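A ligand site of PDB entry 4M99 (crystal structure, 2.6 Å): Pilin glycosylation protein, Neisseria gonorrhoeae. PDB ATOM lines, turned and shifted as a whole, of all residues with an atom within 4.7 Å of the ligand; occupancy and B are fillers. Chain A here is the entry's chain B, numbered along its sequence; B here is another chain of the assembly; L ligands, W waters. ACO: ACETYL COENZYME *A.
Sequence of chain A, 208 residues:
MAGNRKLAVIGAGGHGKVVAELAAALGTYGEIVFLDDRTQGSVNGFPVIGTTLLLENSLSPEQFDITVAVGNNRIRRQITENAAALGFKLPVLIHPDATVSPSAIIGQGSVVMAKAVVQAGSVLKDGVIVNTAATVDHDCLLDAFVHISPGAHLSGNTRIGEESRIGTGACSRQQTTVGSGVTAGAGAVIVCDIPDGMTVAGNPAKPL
An oxygen (O) of the ligand is in hydrogen-bond range of the backbone NH of Gly 156, 2.7 Å away.
The backbone NH of Ala 186 of chain B sits at hydrogen-bond distance from an oxygen (O9P) of the ligand (2.8 Å).
The backbone carbonyl oxygen (O) of Ala 186 of chain B is in hydrogen-bond range of a nitrogen (N6A) of the ligand (2.9 Å).
N of Thr 168 of chain B lies within hydrogen-bond range of O5P of the ligand.
The guanidinium group (NH1) of Arg 173 is in salt-bridge range of an oxygen (O1A) of the ligand, at 3.0 Å.
N1A of the ligand lies close to OD1 of Asn 203 (3.2 Å).
An oxygen (O5P) of the ligand lies within hydrogen-bond range of the guanidinium group (NH1) of Arg 165 of chain B (3.2 Å).
N4P of the ligand lies close to OE1 of Gln 174, 3.3 Å away.
NZ of Lys 206 is in salt-bridge range of O9A of the ligand (3.4 Å).
The side-chain hydroxyl (OG1) of Thr 168 of chain B lies within hydrogen-bond range of the side-chain hydroxyl (OG) of Ser 155, at 2.7 Å.
The backbone carbonyl oxygen of Val 191 sits at hydrogen-bond distance from the guanidinium group of Arg 173 (3.0 Å).
NH1 of Arg 165 of chain B lies within hydrogen-bond range of OG of Ser 149 of chain B, at 3.0 Å.
Merely in contact with the ligand: Asp 137 (3.6 Å), His 138 (3.4 Å), Ser 155 (3.1 Å), Val 191 (3.3 Å), Pro 204 (3.2 Å), Ser 149 of chain B (3.6 Å), Pro 150 of chain B (3.8 Å), Gly 167 of chain B (3.1 Å), Gly 185 of chain B (3.2 Å) and Ala 201 of chain B (3.6 Å).
18 residues have an atom within 4 Å of the ligand: Asp 137, His 138, Ser 155, Gly 156, Arg 173, Gln 174, Val 191, Asn 203, Pro 204, Lys 206, Ser 149 of chain B, Pro 150 of chain B, Arg 165 of chain B, Gly 167 of chain B, Thr 168 of chain B, Gly 185 of chain B, Ala 186 of chain B and Ala 201 of chain B.
The nearest printed residue that does not touch the ligand is Gly 202 of chain B (4.01 Å).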
ATOM      1  N   ASP A 137      -4.798 -13.127  -3.656  1.00  0.00           N
ATOM      2  CA  ASP A 137      -5.959 -13.324  -4.496  1.00  0.00           C
ATOM      3  C   ASP A 137      -6.399 -12.085  -5.250  1.00  0.00           C
ATOM      4  O   ASP A 137      -5.712 -11.067  -5.243  1.00  0.00           O
ATOM      5  CB  ASP A 137      -7.123 -13.959  -3.739  1.00  0.00           C
ATOM      6  CG  ASP A 137      -7.654 -15.174  -4.460  1.00  0.00           C
ATOM      7  OD1 ASP A 137      -8.442 -15.007  -5.427  1.00  0.00           O
ATOM      8  OD2 ASP A 137      -7.259 -16.296  -4.089  1.00  0.00           O
ATOM      9  N   HIS A 138      -7.544 -12.189  -5.932  1.00  0.00           N
ATOM     10  CA  HIS A 138      -7.999 -11.119  -6.810  1.00  0.00           C
ATOM     11  C   HIS A 138      -8.073  -9.767  -6.127  1.00  0.00           C
ATOM     12  O   HIS A 138      -8.536  -9.657  -4.985  1.00  0.00           O
ATOM     13  CB  HIS A 138      -9.340 -11.467  -7.458  1.00  0.00           C
ATOM     14  CG  HIS A 138     -10.449 -11.647  -6.485  1.00  0.00           C
ATOM     15  ND1 HIS A 138     -11.343 -10.642  -6.184  1.00  0.00           N
ATOM     16  CD2 HIS A 138     -10.827 -12.711  -5.744  1.00  0.00           C
ATOM     17  CE1 HIS A 138     -12.223 -11.086  -5.298  1.00  0.00           C
ATOM     18  NE2 HIS A 138     -11.924 -12.333  -5.009  1.00  0.00           N
ATOM     19  N   SER A 155      -6.999 -13.376   1.040  1.00  0.00           N
ATOM     20  CA  SER A 155      -8.268 -13.453   0.337  1.00  0.00           C
ATOM     21  C   SER A 155      -8.411 -12.239  -0.566  1.00  0.00           C
ATOM     22  O   SER A 155      -7.530 -11.382  -0.578  1.00  0.00           O
ATOM     23  CB  SER A 155      -9.429 -13.548   1.302  1.00  0.00           C
ATOM     24  OG  SER A 155      -9.317 -14.703   2.100  1.00  0.00           O
ATOM     25  N   GLY A 156      -9.505 -12.179  -1.322  1.00  0.00           N
ATOM     26  CA  GLY A 156      -9.745 -11.077  -2.236  1.00  0.00           C
ATOM     27  C   GLY A 156      -9.756  -9.721  -1.556  1.00  0.00           C
ATOM     28  O   GLY A 156     -10.159  -9.605  -0.406  1.00  0.00           O
ATOM     29  N   ARG A 173      -8.880 -12.675   5.918  1.00  0.00           N
ATOM     30  CA  ARG A 173     -10.252 -12.633   5.450  1.00  0.00           C
ATOM     31  C   ARG A 173     -10.263 -11.615   4.324  1.00  0.00           C
ATOM     32  O   ARG A 173      -9.377 -10.757   4.260  1.00  0.00           O
ATOM     33  CB  ARG A 173     -11.141 -12.180   6.596  1.00  0.00           C
ATOM     34  CG  ARG A 173     -12.623 -12.320   6.348  1.00  0.00           C
ATOM     35  CD  ARG A 173     -13.419 -11.836   7.559  1.00  0.00           C
ATOM     36  NE  ARG A 173     -13.212 -10.422   7.809  1.00  0.00           N
ATOM     37  CZ  ARG A 173     -13.890  -9.729   8.725  1.00  0.00           C
ATOM     38  NH1 ARG A 173     -14.813 -10.328   9.465  1.00  0.00           N
ATOM     39  NH2 ARG A 173     -13.643  -8.431   8.891  1.00  0.00           N
ATOM     40  N   GLN A 174     -11.236 -11.685   3.424  1.00  0.00           N
ATOM     41  CA  GLN A 174     -11.270 -10.723   2.332  1.00  0.00           C
ATOM     42  C   GLN A 174     -11.549  -9.316   2.859  1.00  0.00           C
ATOM     43  O   GLN A 174     -11.939  -9.156   4.016  1.00  0.00           O
ATOM     44  CB  GLN A 174     -12.298 -11.097   1.255  1.00  0.00           C
ATOM     45  CG  GLN A 174     -13.730 -10.902   1.665  1.00  0.00           C
ATOM     46  CD  GLN A 174     -14.339 -12.166   2.210  1.00  0.00           C
ATOM     47  OE1 GLN A 174     -13.987 -12.621   3.303  1.00  0.00           O
ATOM     48  NE2 GLN A 174     -15.242 -12.768   1.432  1.00  0.00           N
ATOM     49  N   VAL A 189      -3.964 -15.344  11.749  1.00  0.00           N
ATOM     50  CA  VAL A 189      -5.234 -15.320  11.040  1.00  0.00           C
ATOM     51  C   VAL A 189      -5.833 -13.925  11.111  1.00  0.00           C
ATOM     52  O   VAL A 189      -6.500 -13.570  12.076  1.00  0.00           O
ATOM     53  CB  VAL A 189      -6.235 -16.317  11.653  1.00  0.00           C
ATOM     54  CG1 VAL A 189      -7.550 -16.273  10.906  1.00  0.00           C
ATOM     55  CG2 VAL A 189      -5.648 -17.723  11.633  1.00  0.00           C
ATOM     56  N   VAL A 191      -8.286 -11.277  10.640  1.00  0.00           N
ATOM     57  CA  VAL A 191      -9.717 -11.141  10.371  1.00  0.00           C
ATOM     58  C   VAL A 191     -10.264  -9.737  10.626  1.00  0.00           C
ATOM     59  O   VAL A 191     -11.472  -9.531  10.573  1.00  0.00           O
ATOM     60  CB  VAL A 191     -10.530 -12.155  11.183  1.00  0.00           C
ATOM     61  CG1 VAL A 191     -10.183 -13.584  10.723  1.00  0.00           C
ATOM     62  CG2 VAL A 191     -10.271 -11.980  12.672  1.00  0.00           C
ATOM     63  N   ASN A 203      -4.667 -16.838  16.495  1.00  0.00           N
ATOM     64  CA  ASN A 203      -5.926 -17.096  15.806  1.00  0.00           C
ATOM     65  C   ASN A 203      -7.117 -16.662  16.661  1.00  0.00           C
ATOM     66  O   ASN A 203      -7.547 -17.406  17.544  1.00  0.00           O
ATOM     67  CB  ASN A 203      -6.014 -18.600  15.512  1.00  0.00           C
ATOM     68  CG  ASN A 203      -7.231 -18.971  14.694  1.00  0.00           C
ATOM     69  OD1 ASN A 203      -8.107 -18.145  14.427  1.00  0.00           O
ATOM     70  ND2 ASN A 203      -7.301 -20.229  14.291  1.00  0.00           N
ATOM     71  N   PRO A 204      -7.672 -15.459  16.408  1.00  0.00           N
ATOM     72  CA  PRO A 204      -7.314 -14.485  15.369  1.00  0.00           C
ATOM     73  C   PRO A 204      -6.139 -13.617  15.762  1.00  0.00           C
ATOM     74  O   PRO A 204      -5.738 -13.584  16.927  1.00  0.00           O
ATOM     75  CB  PRO A 204      -8.572 -13.624  15.286  1.00  0.00           C
ATOM     76  CG  PRO A 204      -9.073 -13.611  16.688  1.00  0.00           C
ATOM     77  CD  PRO A 204      -8.820 -15.002  17.209  1.00  0.00           C
ATOM     78  N   LYS A 206      -3.977 -10.951  17.055  1.00  0.00           N
ATOM     79  CA  LYS A 206      -4.064  -9.863  18.022  1.00  0.00           C
ATOM     80  C   LYS A 206      -2.658  -9.395  18.309  1.00  0.00           C
ATOM     81  O   LYS A 206      -1.700 -10.142  18.101  1.00  0.00           O
ATOM     82  CB  LYS A 206      -4.776 -10.332  19.291  1.00  0.00           C
ATOM     83  CG  LYS A 206      -6.291 -10.266  19.168  1.00  0.00           C
ATOM     84  CD  LYS A 206      -7.010 -11.059  20.246  1.00  0.00           C
ATOM     85  CE  LYS A 206      -8.521 -10.811  20.167  1.00  0.00           C
ATOM     86  NZ  LYS A 206      -9.328 -11.975  20.624  1.00  0.00           N
ATOM     87  N   ASN B 131     -10.825 -23.363  -4.396  1.00  0.00           N
ATOM     88  CA  ASN B 131     -10.175 -22.110  -4.746  1.00  0.00           C
ATOM     89  C   ASN B 131      -8.651 -22.140  -4.711  1.00  0.00           C
ATOM     90  O   ASN B 131      -8.047 -23.168  -4.418  1.00  0.00           O
ATOM     91  CB  ASN B 131     -10.704 -20.973  -3.869  1.00  0.00           C
ATOM     92  CG  ASN B 131     -11.082 -19.742  -4.688  1.00  0.00           C
ATOM     93  OD1 ASN B 131     -10.327 -19.308  -5.568  1.00  0.00           O
ATOM     94  ND2 ASN B 131     -12.248 -19.170  -4.398  1.00  0.00           N
ATOM     95  N   HIS B 147     -17.883 -24.560  -1.044  1.00  0.00           N
ATOM     96  CA  HIS B 147     -16.777 -23.691  -1.413  1.00  0.00           C
ATOM     97  C   HIS B 147     -15.591 -23.891  -0.467  1.00  0.00           C
ATOM     98  O   HIS B 147     -15.683 -23.645   0.745  1.00  0.00           O
ATOM     99  CB  HIS B 147     -17.239 -22.234  -1.448  1.00  0.00           C
ATOM    100  CG  HIS B 147     -16.157 -21.256  -1.822  1.00  0.00           C
ATOM    101  ND1 HIS B 147     -16.309 -19.903  -1.681  1.00  0.00           N
ATOM    102  CD2 HIS B 147     -14.914 -21.451  -2.310  1.00  0.00           C
ATOM    103  CE1 HIS B 147     -15.211 -19.287  -2.085  1.00  0.00           C
ATOM    104  NE2 HIS B 147     -14.340 -20.207  -2.460  1.00  0.00           N
ATOM    105  N   SER B 149     -12.248 -22.292   0.242  1.00  0.00           N
ATOM    106  CA  SER B 149     -11.582 -21.031  -0.020  1.00  0.00           C
ATOM    107  C   SER B 149     -10.068 -21.214  -0.247  1.00  0.00           C
ATOM    108  O   SER B 149      -9.533 -22.287   0.053  1.00  0.00           O
ATOM    109  CB  SER B 149     -11.837 -20.068   1.160  1.00  0.00           C
ATOM    110  OG  SER B 149     -13.221 -19.896   1.376  1.00  0.00           O
ATOM    111  N   PRO B 150      -9.384 -20.174  -0.763  1.00  0.00           N
ATOM    112  CA  PRO B 150      -7.942 -20.289  -1.025  1.00  0.00           C
ATOM    113  C   PRO B 150      -7.117 -20.843   0.146  1.00  0.00           C
ATOM    114  O   PRO B 150      -7.306 -20.444   1.292  1.00  0.00           O
ATOM    115  CB  PRO B 150      -7.532 -18.851  -1.320  1.00  0.00           C
ATOM    116  CG  PRO B 150      -8.741 -18.290  -2.026  1.00  0.00           C
ATOM    117  CD  PRO B 150      -9.930 -18.903  -1.301  1.00  0.00           C
ATOM    118  N   ARG B 165     -19.045 -23.837   3.690  1.00  0.00           N
ATOM    119  CA  ARG B 165     -18.019 -22.924   3.215  1.00  0.00           C
ATOM    120  C   ARG B 165     -16.781 -23.023   4.075  1.00  0.00           C
ATOM    121  O   ARG B 165     -16.796 -22.618   5.231  1.00  0.00           O
ATOM    122  CB  ARG B 165     -18.537 -21.484   3.272  1.00  0.00           C
ATOM    123  CG  ARG B 165     -17.708 -20.519   2.463  1.00  0.00           C
ATOM    124  CD  ARG B 165     -18.027 -19.074   2.781  1.00  0.00           C
ATOM    125  NE  ARG B 165     -17.521 -18.214   1.722  1.00  0.00           N
ATOM    126  CZ  ARG B 165     -16.258 -17.813   1.616  1.00  0.00           C
ATOM    127  NH1 ARG B 165     -15.355 -18.200   2.507  1.00  0.00           N
ATOM    128  NH2 ARG B 165     -15.891 -17.028   0.602  1.00  0.00           N
ATOM    129  N   GLY B 167     -13.231 -21.709   4.969  1.00  0.00           N
ATOM    130  CA  GLY B 167     -12.572 -20.430   4.798  1.00  0.00           C
ATOM    131  C   GLY B 167     -11.089 -20.502   4.478  1.00  0.00           C
ATOM    132  O   GLY B 167     -10.436 -21.525   4.668  1.00  0.00           O
ATOM    133  N   THR B 168     -10.561 -19.386   3.997  1.00  0.00           N
ATOM    134  CA  THR B 168      -9.173 -19.258   3.584  1.00  0.00           C
ATOM    135  C   THR B 168      -8.188 -19.759   4.646  1.00  0.00           C
ATOM    136  O   THR B 168      -8.172 -19.276   5.766  1.00  0.00           O
ATOM    137  CB  THR B 168      -8.875 -17.800   3.230  1.00  0.00           C
ATOM    138  OG1 THR B 168      -9.667 -17.419   2.099  1.00  0.00           O
ATOM    139  CG2 THR B 168      -7.406 -17.598   2.903  1.00  0.00           C
ATOM    140  N   THR B 183     -20.241 -22.792   8.095  1.00  0.00           N
ATOM    141  CA  THR B 183     -19.280 -21.788   7.691  1.00  0.00           C
ATOM    142  C   THR B 183     -18.099 -21.929   8.625  1.00  0.00           C
ATOM    143  O   THR B 183     -18.190 -21.584   9.821  1.00  0.00           O
ATOM    144  CB  THR B 183     -19.843 -20.343   7.796  1.00  0.00           C
ATOM    145  OG1 THR B 183     -20.783 -20.104   6.739  1.00  0.00           O
ATOM    146  CG2 THR B 183     -18.721 -19.318   7.702  1.00  0.00           C
ATOM    147  N   GLY B 185     -14.536 -20.443   9.241  1.00  0.00           N
ATOM    148  CA  GLY B 185     -13.884 -19.229   8.792  1.00  0.00           C
ATOM    149  C   GLY B 185     -12.407 -19.406   8.509  1.00  0.00           C
ATOM    150  O   GLY B 185     -11.855 -20.476   8.708  1.00  0.00           O
ATOM    151  N   ALA B 186     -11.784 -18.330   8.043  1.00  0.00           N
ATOM    152  CA  ALA B 186     -10.355 -18.310   7.797  1.00  0.00           C
ATOM    153  C   ALA B 186      -9.555 -18.854   8.979  1.00  0.00           C
ATOM    154  O   ALA B 186      -9.753 -18.438  10.109  1.00  0.00           O
ATOM    155  CB  ALA B 186      -9.905 -16.890   7.443  1.00  0.00           C
ATOM    156  N   ALA B 201     -14.866 -21.155  14.066  1.00  0.00           N
ATOM    157  CA  ALA B 201     -13.571 -20.582  13.729  1.00  0.00           C
ATOM    158  C   ALA B 201     -12.655 -20.917  14.880  1.00  0.00           C
ATOM    159  O   ALA B 201     -13.099 -21.488  15.878  1.00  0.00           O
ATOM    160  CB  ALA B 201     -13.665 -19.096  13.526  1.00  0.00           C
ATOM    161  N   GLY B 202     -11.385 -20.573  14.744  1.00  0.00           N
ATOM    162  CA  GLY B 202     -10.422 -20.768  15.811  1.00  0.00           C
ATOM    163  C   GLY B 202      -9.593 -22.035  15.715  1.00  0.00           C
ATOM    164  O   GLY B 202      -9.858 -22.911  14.891  1.00  0.00           O
ATOM    165  N   LEU B 208     -18.603 -19.835  17.385  1.00  0.00           N
ATOM    166  CA  LEU B 208     -18.179 -18.538  17.890  1.00  0.00           C
ATOM    167  C   LEU B 208     -19.131 -18.030  18.976  1.00  0.00           C
ATOM    168  O   LEU B 208     -18.726 -17.335  19.915  1.00  0.00           O
ATOM    169  CB  LEU B 208     -18.057 -17.523  16.741  1.00  0.00           C
ATOM    170  CG  LEU B 208     -16.882 -17.711  15.787  1.00  0.00           C
ATOM    171  CD1 LEU B 208     -16.904 -16.659  14.683  1.00  0.00           C
ATOM    172  CD2 LEU B 208     -15.553 -17.684  16.526  1.00  0.00           C
ATOM    173  OXT LEU B 208     -20.328 -18.339  18.949  1.00  0.00           O
HETATM  174  N1A ACO L   1     -10.856 -16.871  13.259  1.00  0.00           N
HETATM  175  C2A ACO L   1     -10.837 -16.604  14.586  1.00  0.00           C
HETATM  176  N3A ACO L   1     -11.663 -15.728  15.193  1.00  0.00           N
HETATM  177  C4A ACO L   1     -12.584 -15.032  14.479  1.00  0.00           C
HETATM  178  C5A ACO L   1     -12.656 -15.257  13.023  1.00  0.00           C
HETATM  179  C6A ACO L   1     -11.720 -16.247  12.415  1.00  0.00           C
HETATM  180  N6A ACO L   1     -11.740 -16.504  11.086  1.00  0.00           N
HETATM  181  N7A ACO L   1     -13.638 -14.459  12.547  1.00  0.00           N
HETATM  182  C8A ACO L   1     -14.144 -13.777  13.602  1.00  0.00           C
HETATM  183  N9A ACO L   1     -13.520 -14.108  14.748  1.00  0.00           N
HETATM  184  C1B ACO L   1     -13.870 -13.533  16.080  1.00  0.00           C
HETATM  185  C2B ACO L   1     -12.960 -12.387  16.494  1.00  0.00           C
HETATM  186  O2B ACO L   1     -12.028 -12.813  17.485  1.00  0.00           O
HETATM  187  C3B ACO L   1     -13.879 -11.365  17.102  1.00  0.00           C
HETATM  188  O3B ACO L   1     -14.033 -11.642  18.488  1.00  0.00           O
HETATM  189  P3B ACO L   1     -13.829 -10.544  19.648  1.00  0.00           P
HETATM  190  O7A ACO L   1     -13.813  -9.207  18.942  1.00  0.00           O
HETATM  191  O8A ACO L   1     -15.044 -10.776  20.502  1.00  0.00           O
HETATM  192  O9A ACO L   1     -12.520 -10.954  20.296  1.00  0.00           O
HETATM  193  C4B ACO L   1     -15.223 -11.640  16.463  1.00  0.00           C
HETATM  194  O4B ACO L   1     -15.199 -12.995  15.998  1.00  0.00           O
HETATM  195  C5B ACO L   1     -15.471 -10.702  15.288  1.00  0.00           C
HETATM  196  O5B ACO L   1     -16.588 -11.195  14.585  1.00  0.00           O
HETATM  197  P1A ACO L   1     -16.952 -10.728  13.083  1.00  0.00           P
HETATM  198  O1A ACO L   1     -15.654 -10.409  12.377  1.00  0.00           O
HETATM  199  O2A ACO L   1     -18.059  -9.698  13.124  1.00  0.00           O
HETATM  200  O3A ACO L   1     -17.536 -12.132  12.568  1.00  0.00           O
HETATM  201  P2A ACO L   1     -18.644 -12.304  11.412  1.00  0.00           P
HETATM  202  O4A ACO L   1     -19.985 -12.575  12.065  1.00  0.00           O
HETATM  203  O5A ACO L   1     -18.482 -11.186  10.407  1.00  0.00           O
HETATM  204  O6A ACO L   1     -18.132 -13.676  10.750  1.00  0.00           O
HETATM  205  CBP ACO L   1     -16.327 -15.077   9.861  1.00  0.00           C
HETATM  206  CCP ACO L   1     -16.742 -13.974  10.832  1.00  0.00           C
HETATM  207  CDP ACO L   1     -17.467 -15.389   8.889  1.00  0.00           C
HETATM  208  CEP ACO L   1     -15.945 -16.335  10.644  1.00  0.00           C
HETATM  209  CAP ACO L   1     -15.099 -14.522   9.137  1.00  0.00           C
HETATM  210  OAP ACO L   1     -14.227 -13.908  10.095  1.00  0.00           O
HETATM  211  C9P ACO L   1     -14.353 -15.546   8.329  1.00  0.00           C
HETATM  212  O9P ACO L   1     -13.328 -16.060   8.770  1.00  0.00           O
HETATM  213  N8P ACO L   1     -14.845 -15.828   7.125  1.00  0.00           N
HETATM  214  C7P ACO L   1     -14.015 -16.407   6.099  1.00  0.00           C
HETATM  215  C6P ACO L   1     -13.727 -15.450   4.946  1.00  0.00           C
HETATM  216  C5P ACO L   1     -12.978 -16.234   3.898  1.00  0.00           C
HETATM  217  O5P ACO L   1     -12.695 -17.398   4.094  1.00  0.00           O
HETATM  218  N4P ACO L   1     -12.673 -15.617   2.776  1.00  0.00           N
HETATM  219  C3P ACO L   1     -12.735 -16.324   1.520  1.00  0.00           C
HETATM  220  C2P ACO L   1     -12.515 -15.351   0.376  1.00  0.00           C
HETATM  221  S1P ACO L   1     -12.647 -16.190  -1.165  1.00  0.00           S
HETATM  222  C   ACO L   1     -11.537 -15.255  -1.988  1.00  0.00           C
HETATM  223  O   ACO L   1     -10.814 -14.491  -1.356  1.00  0.00           O
HETATM  224  CH3 ACO L   1     -11.439 -15.350  -3.478  1.00  0.00           C
HETATM  225  O   HOH W   1     -21.513 -10.209   9.679  1.00  0.00           O
HETATM  226  O   HOH W   2     -16.637 -13.683   5.934  1.00  0.00           O
HETATM  227  O   HOH W   3     -12.695 -16.606  -5.959  1.00  0.00           O
HETATM  228  O   HOH W   4      -9.720 -19.743  12.709  1.00  0.00           O
